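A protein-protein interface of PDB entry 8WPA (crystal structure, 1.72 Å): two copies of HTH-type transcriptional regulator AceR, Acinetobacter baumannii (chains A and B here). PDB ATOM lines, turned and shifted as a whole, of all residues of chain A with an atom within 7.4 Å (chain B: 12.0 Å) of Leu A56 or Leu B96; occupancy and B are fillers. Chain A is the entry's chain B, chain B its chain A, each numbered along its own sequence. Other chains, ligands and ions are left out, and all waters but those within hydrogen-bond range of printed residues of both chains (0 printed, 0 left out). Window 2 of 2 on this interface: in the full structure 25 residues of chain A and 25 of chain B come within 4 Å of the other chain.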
ATOM      1  N   ILE A  47      -5.037 -15.816  19.874  1.00  0.00           N
ATOM      2  CA  ILE A  47      -5.498 -15.884  18.497  1.00  0.00           C
ATOM      3  C   ILE A  47      -6.870 -15.236  18.363  1.00  0.00           C
ATOM      4  O   ILE A  47      -7.103 -14.467  17.435  1.00  0.00           O
ATOM      5  CB  ILE A  47      -5.530 -17.330  17.955  1.00  0.00           C
ATOM      6  CG1 ILE A  47      -4.094 -17.923  17.884  1.00  0.00           C
ATOM      7  CG2 ILE A  47      -6.210 -17.406  16.629  1.00  0.00           C
ATOM      8  CD1 ILE A  47      -3.137 -17.198  16.968  1.00  0.00           C
ATOM      9  N   ALA A  48      -7.773 -15.518  19.320  1.00  0.00           N
ATOM     10  CA  ALA A  48      -9.075 -14.877  19.288  1.00  0.00           C
ATOM     11  C   ALA A  48      -8.924 -13.353  19.327  1.00  0.00           C
ATOM     12  O   ALA A  48      -9.566 -12.650  18.542  1.00  0.00           O
ATOM     13  CB  ALA A  48      -9.933 -15.357  20.451  1.00  0.00           C
ATOM     14  N   LEU A  50      -6.337 -11.564  18.460  1.00  0.00           N
ATOM     15  CA  LEU A  50      -5.769 -11.118  17.199  1.00  0.00           C
ATOM     16  C   LEU A  50      -6.823 -10.988  16.101  1.00  0.00           C
ATOM     17  O   LEU A  50      -6.816 -10.002  15.356  1.00  0.00           O
ATOM     18  CB  LEU A  50      -4.659 -12.090  16.775  1.00  0.00           C
ATOM     19  CG  LEU A  50      -3.944 -11.767  15.485  1.00  0.00           C
ATOM     20  CD1 LEU A  50      -3.264 -10.415  15.531  1.00  0.00           C
ATOM     21  CD2 LEU A  50      -2.911 -12.825  15.188  1.00  0.00           C
ATOM     22  N   GLU A  51      -7.722 -11.984  15.997  1.00  0.00           N
ATOM     23  CA  GLU A  51      -8.795 -11.952  15.024  1.00  0.00           C
ATOM     24  C   GLU A  51      -9.688 -10.739  15.251  1.00  0.00           C
ATOM     25  O   GLU A  51     -10.082 -10.070  14.302  1.00  0.00           O
ATOM     26  CB  GLU A  51      -9.621 -13.222  15.064  1.00  0.00           C
ATOM     27  CG  GLU A  51      -8.883 -14.469  14.589  1.00  0.00           C
ATOM     28  CD  GLU A  51      -9.731 -15.724  14.553  1.00  0.00           C
ATOM     29  OE1 GLU A  51     -10.448 -15.940  15.558  1.00  0.00           O
ATOM     30  OE2 GLU A  51      -9.689 -16.496  13.561  1.00  0.00           O
ATOM     31  N   ILE A  52      -9.971 -10.459  16.529  1.00  0.00           N
ATOM     32  CA  ILE A  52     -10.765  -9.284  16.862  1.00  0.00           C
ATOM     33  C   ILE A  52     -10.089  -7.983  16.435  1.00  0.00           C
ATOM     34  O   ILE A  52     -10.725  -7.134  15.792  1.00  0.00           O
ATOM     35  CB  ILE A  52     -11.134  -9.328  18.373  1.00  0.00           C
ATOM     36  CG1 ILE A  52     -11.992 -10.525  18.670  1.00  0.00           C
ATOM     37  CG2 ILE A  52     -11.813  -8.009  18.815  1.00  0.00           C
ATOM     38  CD1 ILE A  52     -12.103 -10.855  20.152  1.00  0.00           C
ATOM     39  N   ASP A  53      -8.801  -7.823  16.781  1.00  0.00           N
ATOM     40  CA  ASP A  53      -8.040  -6.613  16.493  1.00  0.00           C
ATOM     41  C   ASP A  53      -7.884  -6.370  14.986  1.00  0.00           C
ATOM     42  O   ASP A  53      -7.947  -5.223  14.530  1.00  0.00           O
ATOM     43  CB  ASP A  53      -6.646  -6.650  17.135  1.00  0.00           C
ATOM     44  CG  ASP A  53      -6.533  -6.626  18.646  1.00  0.00           C
ATOM     45  OD1 ASP A  53      -7.491  -6.173  19.308  1.00  0.00           O
ATOM     46  OD2 ASP A  53      -5.477  -7.078  19.174  1.00  0.00           O
ATOM     47  N   LEU A  54      -7.674  -7.450  14.217  1.00  0.00           N
ATOM     48  CA  LEU A  54      -7.571  -7.361  12.770  1.00  0.00           C
ATOM     49  C   LEU A  54      -8.910  -7.355  12.045  1.00  0.00           C
ATOM     50  O   LEU A  54      -8.974  -7.029  10.858  1.00  0.00           O
ATOM     51  CB  LEU A  54      -6.793  -8.565  12.215  1.00  0.00           C
ATOM     52  CG  LEU A  54      -5.368  -8.679  12.665  1.00  0.00           C
ATOM     53  CD1 LEU A  54      -4.680  -9.827  12.016  1.00  0.00           C
ATOM     54  CD2 LEU A  54      -4.590  -7.402  12.377  1.00  0.00           C
ATOM     55  N   ASN A  55      -9.962  -7.749  12.770  1.00  0.00           N
ATOM     56  CA  ASN A  55     -11.263  -8.042  12.203  1.00  0.00           C
ATOM     57  C   ASN A  55     -11.138  -8.978  10.998  1.00  0.00           C
ATOM     58  O   ASN A  55     -11.712  -8.702   9.946  1.00  0.00           O
ATOM     59  CB  ASN A  55     -12.004  -6.740  11.856  1.00  0.00           C
ATOM     60  CG  ASN A  55     -13.467  -6.944  11.710  1.00  0.00           C
ATOM     61  OD1 ASN A  55     -14.088  -7.721  12.443  1.00  0.00           O
ATOM     62  ND2 ASN A  55     -14.063  -6.286  10.740  1.00  0.00           N
ATOM     63  N   LEU A  56     -10.362 -10.059  11.180  1.00  0.00           N
ATOM     64  CA  LEU A  56     -10.182 -11.105  10.173  1.00  0.00           C
ATOM     65  C   LEU A  56     -10.299 -12.484  10.815  1.00  0.00           C
ATOM     66  O   LEU A  56      -9.740 -12.701  11.890  1.00  0.00           O
ATOM     67  CB  LEU A  56      -8.775 -11.058   9.537  1.00  0.00           C
ATOM     68  CG  LEU A  56      -8.397  -9.905   8.650  1.00  0.00           C
ATOM     69  CD1 LEU A  56      -6.904 -10.027   8.263  1.00  0.00           C
ATOM     70  CD2 LEU A  56      -9.269  -9.840   7.406  1.00  0.00           C
ATOM     71  N   THR A  57     -10.997 -13.415  10.147  1.00  0.00           N
ATOM     72  CA  THR A  57     -11.001 -14.799  10.590  1.00  0.00           C
ATOM     73  C   THR A  57      -9.745 -15.462  10.030  1.00  0.00           C
ATOM     74  O   THR A  57      -9.485 -15.399   8.837  1.00  0.00           O
ATOM     75  CB  THR A  57     -12.253 -15.515  10.171  1.00  0.00           C
ATOM     76  OG1 THR A  57     -13.371 -14.875  10.846  1.00  0.00           O
ATOM     77  CG2 THR A  57     -12.192 -17.012  10.509  1.00  0.00           C
ATOM     78  N   LEU A  58      -8.948 -16.026  10.937  1.00  0.00           N
ATOM     79  CA  LEU A  58      -7.635 -16.544  10.610  1.00  0.00           C
ATOM     80  C   LEU A  58      -7.664 -18.063  10.501  1.00  0.00           C
ATOM     81  O   LEU A  58      -6.833 -18.637   9.807  1.00  0.00           O
ATOM     82  CB  LEU A  58      -6.596 -16.110  11.630  1.00  0.00           C
ATOM     83  CG  LEU A  58      -6.288 -14.570  11.608  1.00  0.00           C
ATOM     84  CD1 LEU A  58      -5.367 -14.185  12.742  1.00  0.00           C
ATOM     85  CD2 LEU A  58      -5.722 -14.151  10.215  1.00  0.00           C
ATOM     86  N   PHE A  59      -8.603 -18.713  11.209  1.00  0.00           N
ATOM     87  CA  PHE A  59      -8.687 -20.168  11.207  1.00  0.00           C
ATOM     88  C   PHE A  59     -10.152 -20.579  11.106  1.00  0.00           C
ATOM     89  O   PHE A  59     -11.018 -19.937  11.699  1.00  0.00           O
ATOM     90  CB  PHE A  59      -8.038 -20.777  12.457  1.00  0.00           C
ATOM     91  CG  PHE A  59      -6.587 -20.427  12.575  1.00  0.00           C
ATOM     92  CD1 PHE A  59      -5.633 -21.109  11.845  1.00  0.00           C
ATOM     93  CD2 PHE A  59      -6.175 -19.353  13.351  1.00  0.00           C
ATOM     94  CE1 PHE A  59      -4.298 -20.733  11.900  1.00  0.00           C
ATOM     95  CE2 PHE A  59      -4.830 -19.000  13.416  1.00  0.00           C
ATOM     96  CZ  PHE A  59      -3.912 -19.680  12.665  1.00  0.00           C
ATOM     97  N   THR A  69      -7.082 -19.710   7.093  1.00  0.00           N
ATOM     98  CA  THR A  69      -7.741 -19.074   5.968  1.00  0.00           C
ATOM     99  C   THR A  69      -6.699 -18.562   4.977  1.00  0.00           C
ATOM    100  O   THR A  69      -5.503 -18.490   5.282  1.00  0.00           O
ATOM    101  CB  THR A  69      -8.636 -17.918   6.437  1.00  0.00           C
ATOM    102  OG1 THR A  69      -7.789 -16.942   7.070  1.00  0.00           O
ATOM    103  CG2 THR A  69      -9.734 -18.380   7.362  1.00  0.00           C
ATOM    104  N   ALA A  70      -7.175 -18.169   3.790  1.00  0.00           N
ATOM    105  CA  ALA A  70      -6.309 -17.578   2.783  1.00  0.00           C
ATOM    106  C   ALA A  70      -5.616 -16.330   3.330  1.00  0.00           C
ATOM    107  O   ALA A  70      -4.424 -16.103   3.078  1.00  0.00           O
ATOM    108  CB  ALA A  70      -7.093 -17.232   1.537  1.00  0.00           C
ATOM    109  N   GLU A  71      -6.376 -15.542   4.099  1.00  0.00           N
ATOM    110  CA  GLU A  71      -5.852 -14.321   4.690  1.00  0.00           C
ATOM    111  C   GLU A  71      -4.739 -14.617   5.690  1.00  0.00           C
ATOM    112  O   GLU A  71      -3.747 -13.898   5.740  1.00  0.00           O
ATOM    113  CB  GLU A  71      -6.983 -13.521   5.367  1.00  0.00           C
ATOM    114  CG  GLU A  71      -7.993 -12.935   4.396  1.00  0.00           C
ATOM    115  CD  GLU A  71      -9.023 -13.890   3.796  1.00  0.00           C
ATOM    116  OE1 GLU A  71      -9.139 -15.035   4.292  1.00  0.00           O
ATOM    117  OE2 GLU A  71      -9.693 -13.499   2.812  1.00  0.00           O
ATOM    118  N   ALA A  72      -4.914 -15.670   6.499  1.00  0.00           N
ATOM    119  CA  ALA A  72      -3.869 -16.085   7.417  1.00  0.00           C
ATOM    120  C   ALA A  72      -2.567 -16.447   6.694  1.00  0.00           C
ATOM    121  O   ALA A  72      -1.466 -16.177   7.187  1.00  0.00           O
ATOM    122  CB  ALA A  72      -4.359 -17.261   8.266  1.00  0.00           C
ATOM    123  N   ARG A  73      -2.698 -17.102   5.545  1.00  0.00           N
ATOM    124  CA  ARG A  73      -1.536 -17.510   4.763  1.00  0.00           C
ATOM    125  C   ARG A  73      -0.672 -16.297   4.457  1.00  0.00           C
ATOM    126  O   ARG A  73       0.528 -16.285   4.727  1.00  0.00           O
ATOM    127  CB  ARG A  73      -1.974 -18.189   3.465  1.00  0.00           C
ATOM    128  CG  ARG A  73      -1.970 -19.708   3.526  1.00  0.00           C
ATOM    129  CD  ARG A  73      -2.597 -20.312   2.278  1.00  0.00           C
ATOM    130  NE  ARG A  73      -3.285 -21.568   2.564  1.00  0.00           N
ATOM    131  CZ  ARG A  73      -2.773 -22.549   3.300  1.00  0.00           C
ATOM    132  NH1 ARG A  73      -1.563 -22.422   3.829  1.00  0.00           N
ATOM    133  NH2 ARG A  73      -3.469 -23.658   3.508  1.00  0.00           N
ATOM    134  N   VAL A  74      -1.302 -15.276   3.888  1.00  0.00           N
ATOM    135  CA  VAL A  74      -0.621 -14.035   3.546  1.00  0.00           C
ATOM    136  C   VAL A  74      -0.071 -13.327   4.788  1.00  0.00           C
ATOM    137  O   VAL A  74       1.051 -12.822   4.791  1.00  0.00           O
ATOM    138  CB  VAL A  74      -1.545 -13.116   2.749  1.00  0.00           C
ATOM    139  CG1 VAL A  74      -0.891 -11.761   2.506  1.00  0.00           C
ATOM    140  CG2 VAL A  74      -2.006 -13.775   1.445  1.00  0.00           C
ATOM    141  N   LEU A  75      -0.880 -13.270   5.849  1.00  0.00           N
ATOM    142  CA  LEU A  75      -0.453 -12.609   7.063  1.00  0.00           C
ATOM    143  C   LEU A  75       0.782 -13.274   7.663  1.00  0.00           C
ATOM    144  O   LEU A  75       1.634 -12.583   8.214  1.00  0.00           O
ATOM    145  CB  LEU A  75      -1.611 -12.589   8.077  1.00  0.00           C
ATOM    146  CG  LEU A  75      -1.355 -11.851   9.365  1.00  0.00           C
ATOM    147  CD1 LEU A  75      -1.199 -10.422   9.097  1.00  0.00           C
ATOM    148  CD2 LEU A  75      -2.456 -12.140  10.376  1.00  0.00           C
ATOM    149  N   TYR A  76       0.918 -14.604   7.547  1.00  0.00           N
ATOM    150  CA  TYR A  76       2.119 -15.281   8.017  1.00  0.00           C
ATOM    151  C   TYR A  76       3.391 -14.677   7.381  1.00  0.00           C
ATOM    152  O   TYR A  76       4.396 -14.434   8.073  1.00  0.00           O
ATOM    153  CB  TYR A  76       2.103 -16.823   7.732  1.00  0.00           C
ATOM    154  CG  TYR A  76       3.383 -17.474   8.197  1.00  0.00           C
ATOM    155  CD1 TYR A  76       3.592 -17.752   9.529  1.00  0.00           C
ATOM    156  CD2 TYR A  76       4.411 -17.766   7.308  1.00  0.00           C
ATOM    157  CE1 TYR A  76       4.774 -18.337   9.971  1.00  0.00           C
ATOM    158  CE2 TYR A  76       5.623 -18.288   7.753  1.00  0.00           C
ATOM    159  CZ  TYR A  76       5.802 -18.573   9.084  1.00  0.00           C
ATOM    160  OH  TYR A  76       6.976 -19.113   9.585  1.00  0.00           O
ATOM    161  N   LYS A  78       3.876 -11.715   5.919  1.00  0.00           N
ATOM    162  CA  LYS A  78       4.124 -10.330   6.290  1.00  0.00           C
ATOM    163  C   LYS A  78       4.582 -10.230   7.740  1.00  0.00           C
ATOM    164  O   LYS A  78       5.415  -9.396   8.076  1.00  0.00           O
ATOM    165  CB  LYS A  78       2.902  -9.487   6.064  1.00  0.00           C
ATOM    166  CG  LYS A  78       2.265  -9.620   4.684  1.00  0.00           C
ATOM    167  CD  LYS A  78       3.253  -9.400   3.566  1.00  0.00           C
ATOM    168  CE  LYS A  78       2.590  -9.483   2.212  1.00  0.00           C
ATOM    169  NZ  LYS A  78       3.610  -9.505   1.156  1.00  0.00           N
ATOM    170  N   ASN B  87       4.313  -0.045   9.964  1.00  0.00           N
ATOM    171  CA  ASN B  87       3.381   0.618   9.071  1.00  0.00           C
ATOM    172  C   ASN B  87       3.065  -0.205   7.816  1.00  0.00           C
ATOM    173  O   ASN B  87       1.904  -0.281   7.402  1.00  0.00           O
ATOM    174  CB  ASN B  87       3.849   2.021   8.736  1.00  0.00           C
ATOM    175  CG  ASN B  87       2.714   2.755   8.026  1.00  0.00           C
ATOM    176  OD1 ASN B  87       1.740   3.167   8.649  1.00  0.00           O
ATOM    177  ND2 ASN B  87       2.740   2.771   6.755  1.00  0.00           N
ATOM    178  N   GLN B  88       4.089  -0.839   7.244  1.00  0.00           N
ATOM    179  CA  GLN B  88       3.901  -1.644   6.055  1.00  0.00           C
ATOM    180  C   GLN B  88       3.028  -2.863   6.381  1.00  0.00           C
ATOM    181  O   GLN B  88       2.134  -3.240   5.605  1.00  0.00           O
ATOM    182  CB  GLN B  88       5.253  -2.132   5.467  1.00  0.00           C
ATOM    183  CG  GLN B  88       6.318  -1.053   5.239  1.00  0.00           C
ATOM    184  CD  GLN B  88       6.395  -0.409   3.886  1.00  0.00           C
ATOM    185  OE1 GLN B  88       7.046   0.657   3.728  1.00  0.00           O
ATOM    186  NE2 GLN B  88       5.774  -1.030   2.886  1.00  0.00           N
ATOM    187  N   TRP B  89       3.301  -3.479   7.537  1.00  0.00           N
ATOM    188  CA  TRP B  89       2.512  -4.615   7.981  1.00  0.00           C
ATOM    189  C   TRP B  89       1.027  -4.263   8.142  1.00  0.00           C
ATOM    190  O   TRP B  89       0.149  -4.968   7.674  1.00  0.00           O
ATOM    191  CB  TRP B  89       3.090  -5.130   9.287  1.00  0.00           C
ATOM    192  CG  TRP B  89       2.405  -6.340   9.810  1.00  0.00           C
ATOM    193  CD1 TRP B  89       2.690  -7.625   9.509  1.00  0.00           C
ATOM    194  CD2 TRP B  89       1.296  -6.366  10.716  1.00  0.00           C
ATOM    195  NE1 TRP B  89       1.882  -8.476  10.236  1.00  0.00           N
ATOM    196  CE2 TRP B  89       1.010  -7.721  10.983  1.00  0.00           C
ATOM    197  CE3 TRP B  89       0.573  -5.378  11.382  1.00  0.00           C
ATOM    198  CZ2 TRP B  89      -0.023  -8.115  11.827  1.00  0.00           C
ATOM    199  CZ3 TRP B  89      -0.427  -5.779  12.262  1.00  0.00           C
ATOM    200  CH2 TRP B  89      -0.716  -7.138  12.457  1.00  0.00           C
ATOM    201  N   LYS B  90       0.756  -3.126   8.772  1.00  0.00           N
ATOM    202  CA  LYS B  90      -0.606  -2.657   8.961  1.00  0.00           C
ATOM    203  C   LYS B  90      -1.306  -2.420   7.631  1.00  0.00           C
ATOM    204  O   LYS B  90      -2.494  -2.711   7.488  1.00  0.00           O
ATOM    205  CB  LYS B  90      -0.604  -1.370   9.792  1.00  0.00           C
ATOM    206  CG  LYS B  90      -1.981  -0.782  10.009  1.00  0.00           C
ATOM    207  CD  LYS B  90      -1.998   0.237  11.088  1.00  0.00           C
ATOM    208  CE  LYS B  90      -1.394   1.526  10.650  1.00  0.00           C
ATOM    209  NZ  LYS B  90      -1.429   2.539  11.745  1.00  0.00           N
ATOM    210  N   GLN B  91      -0.581  -1.893   6.633  1.00  0.00           N
ATOM    211  CA  GLN B  91      -1.181  -1.672   5.322  1.00  0.00           C
ATOM    212  C   GLN B  91      -1.607  -3.002   4.706  1.00  0.00           C
ATOM    213  O   GLN B  91      -2.705  -3.112   4.139  1.00  0.00           O
ATOM    214  CB  GLN B  91      -0.221  -0.924   4.403  1.00  0.00           C
ATOM    215  CG  GLN B  91      -0.063   0.546   4.835  1.00  0.00           C
ATOM    216  CD  GLN B  91       1.045   1.320   4.096  1.00  0.00           C
ATOM    217  OE1 GLN B  91       1.166   2.542   4.237  1.00  0.00           O
ATOM    218  NE2 GLN B  91       1.879   0.651   3.325  1.00  0.00           N
ATOM    219  N   HIS B  92      -0.747  -4.015   4.840  1.00  0.00           N
ATOM    220  CA  HIS B  92      -1.058  -5.344   4.342  1.00  0.00           C
ATOM    221  C   HIS B  92      -2.266  -5.920   5.081  1.00  0.00           C
ATOM    222  O   HIS B  92      -3.154  -6.492   4.460  1.00  0.00           O
ATOM    223  CB  HIS B  92       0.155  -6.274   4.467  1.00  0.00           C
ATOM    224  CG  HIS B  92       1.265  -5.954   3.534  1.00  0.00           C
ATOM    225  ND1 HIS B  92       1.117  -5.963   2.161  1.00  0.00           N
ATOM    226  CD2 HIS B  92       2.543  -5.624   3.777  1.00  0.00           C
ATOM    227  CE1 HIS B  92       2.270  -5.629   1.603  1.00  0.00           C
ATOM    228  NE2 HIS B  92       3.148  -5.420   2.563  1.00  0.00           N
ATOM    229  N   ALA B  93      -2.282  -5.781   6.413  1.00  0.00           N
ATOM    230  CA  ALA B  93      -3.388  -6.278   7.221  1.00  0.00           C
ATOM    231  C   ALA B  93      -4.713  -5.619   6.844  1.00  0.00           C
ATOM    232  O   ALA B  93      -5.742  -6.287   6.782  1.00  0.00           O
ATOM    233  CB  ALA B  93      -3.102  -6.083   8.708  1.00  0.00           C
ATOM    234  N   HIS B  94      -4.686  -4.312   6.562  1.00  0.00           N
ATOM    235  CA  HIS B  94      -5.891  -3.581   6.186  1.00  0.00           C
ATOM    236  C   HIS B  94      -6.431  -4.064   4.842  1.00  0.00           C
ATOM    237  O   HIS B  94      -7.641  -4.044   4.623  1.00  0.00           O
ATOM    238  CB  HIS B  94      -5.646  -2.074   6.202  1.00  0.00           C
ATOM    239  CG  HIS B  94      -5.790  -1.469   7.557  1.00  0.00           C
ATOM    240  ND1 HIS B  94      -5.110  -0.324   7.912  1.00  0.00           N
ATOM    241  CD2 HIS B  94      -6.502  -1.826   8.633  1.00  0.00           C
ATOM    242  CE1 HIS B  94      -5.437   0.010   9.153  1.00  0.00           C
ATOM    243  NE2 HIS B  94      -6.261  -0.900   9.616  1.00  0.00           N
ATOM    244  N   ALA B  95      -5.535  -4.506   3.955  1.00  0.00           N
ATOM    245  CA  ALA B  95      -5.907  -4.912   2.608  1.00  0.00           C
ATOM    246  C   ALA B  95      -6.484  -6.325   2.515  1.00  0.00           C
ATOM    247  O   ALA B  95      -7.055  -6.682   1.488  1.00  0.00           O
ATOM    248  CB  ALA B  95      -4.697  -4.793   1.695  1.00  0.00           C
ATOM    249  N   LEU B  96      -6.312  -7.137   3.566  1.00  0.00           N
ATOM    250  CA  LEU B  96      -6.823  -8.497   3.562  1.00  0.00           C
ATOM    251  C   LEU B  96      -8.351  -8.546   3.751  1.00  0.00           C
ATOM    252  O   LEU B  96      -8.983  -9.361   3.105  1.00  0.00           O
ATOM    253  CB  LEU B  96      -6.134  -9.324   4.638  1.00  0.00           C
ATOM    254  CG  LEU B  96      -4.669  -9.628   4.340  1.00  0.00           C
ATOM    255  CD1 LEU B  96      -4.023 -10.330   5.487  1.00  0.00           C
ATOM    256  CD2 LEU B  96      -4.537 -10.446   3.070  1.00  0.00           C
ATOM    257  OXT LEU B  96      -8.944  -7.804   4.533  1.00  0.00           O
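The backbone NH (N) of Leu A56 lies within hydrogen-bond range of the backbone carbonyl oxygen (O) of Glu A51 (3.1 Å).
Trp B89 touches Leu A54 (CH2 to CD2, 3.9 Å). Leu B96 touches Leu A56 (OXT to CD2, 3.5 Å). O of Glu A71 touches CD1 of Leu B96, at 3.6 Å. Val A74 touches Leu B96 (CG1 to CD2, 3.9 Å). Trp B89 touches Leu A75 (CZ2 to CD1, 3.8 Å). Lys A78 touches Trp B89 (O to CD1, 3.6 Å). His B92 touches Lys A78 (ND1 to CE, 3.8 Å).
No residue of chain B comes within 4 Å of Glu A51. Of the printed residues of chain B, Leu A54 touches Trp B89 (3.9 Å). No residue of chain B comes within 4 Å of Asn A55. Of chain B, only Leu B96 comes within 4 Å of Leu A56. Thr A57 touches none of the printed residues of chain B. Glu A71 touches one residue of chain B. Ala A72 touches none of the printed residues of chain B. Printed residues of chain B within 4 Å of Val A74: Leu B96. Leu A75 touches one residue of chain B. Printed residues of chain B within 4 Å of Lys A78: Trp B89 (3.6 Å) and His B92 (3.8 Å). Printed residues of chain A within 4 Å of Trp B89: Leu A54 (3.9 Å), Leu A75 (3.8 Å) and Lys A78 (3.6 Å). Of the printed residues of chain A, His B92 touches Lys A78. Of chain A, only Leu A56, Glu A71 and Val A74 come within 4 Å of Leu B96. The nearest residue of chain A that does not touch Leu B96 is Leu A75 (4.2 Å).
Printed residues of chain B that touch a printed residue of chain A: Trp B89, His B92 and Leu B96. Hydrophobic or aromatic side chains of chain B that line the printed part of chain A: Trp B89, His B92 and Leu B96. Hydrophobic or aromatic side chains of chain A within 4 Å of the printed part of chain B: Leu A54, Leu A56, Val A74 and Leu A75. Among the printed residues, 7 pairs touch across the chains. Among the printed residues, no Asp or Glu carboxylate lies within 4 Å of a Lys or Arg side-chain nitrogen of the other chain.
No position is printed for both chains. Of the 7 pairs that touch across the chains among the printed residues, none has its exchanged pair printed and touching as well.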
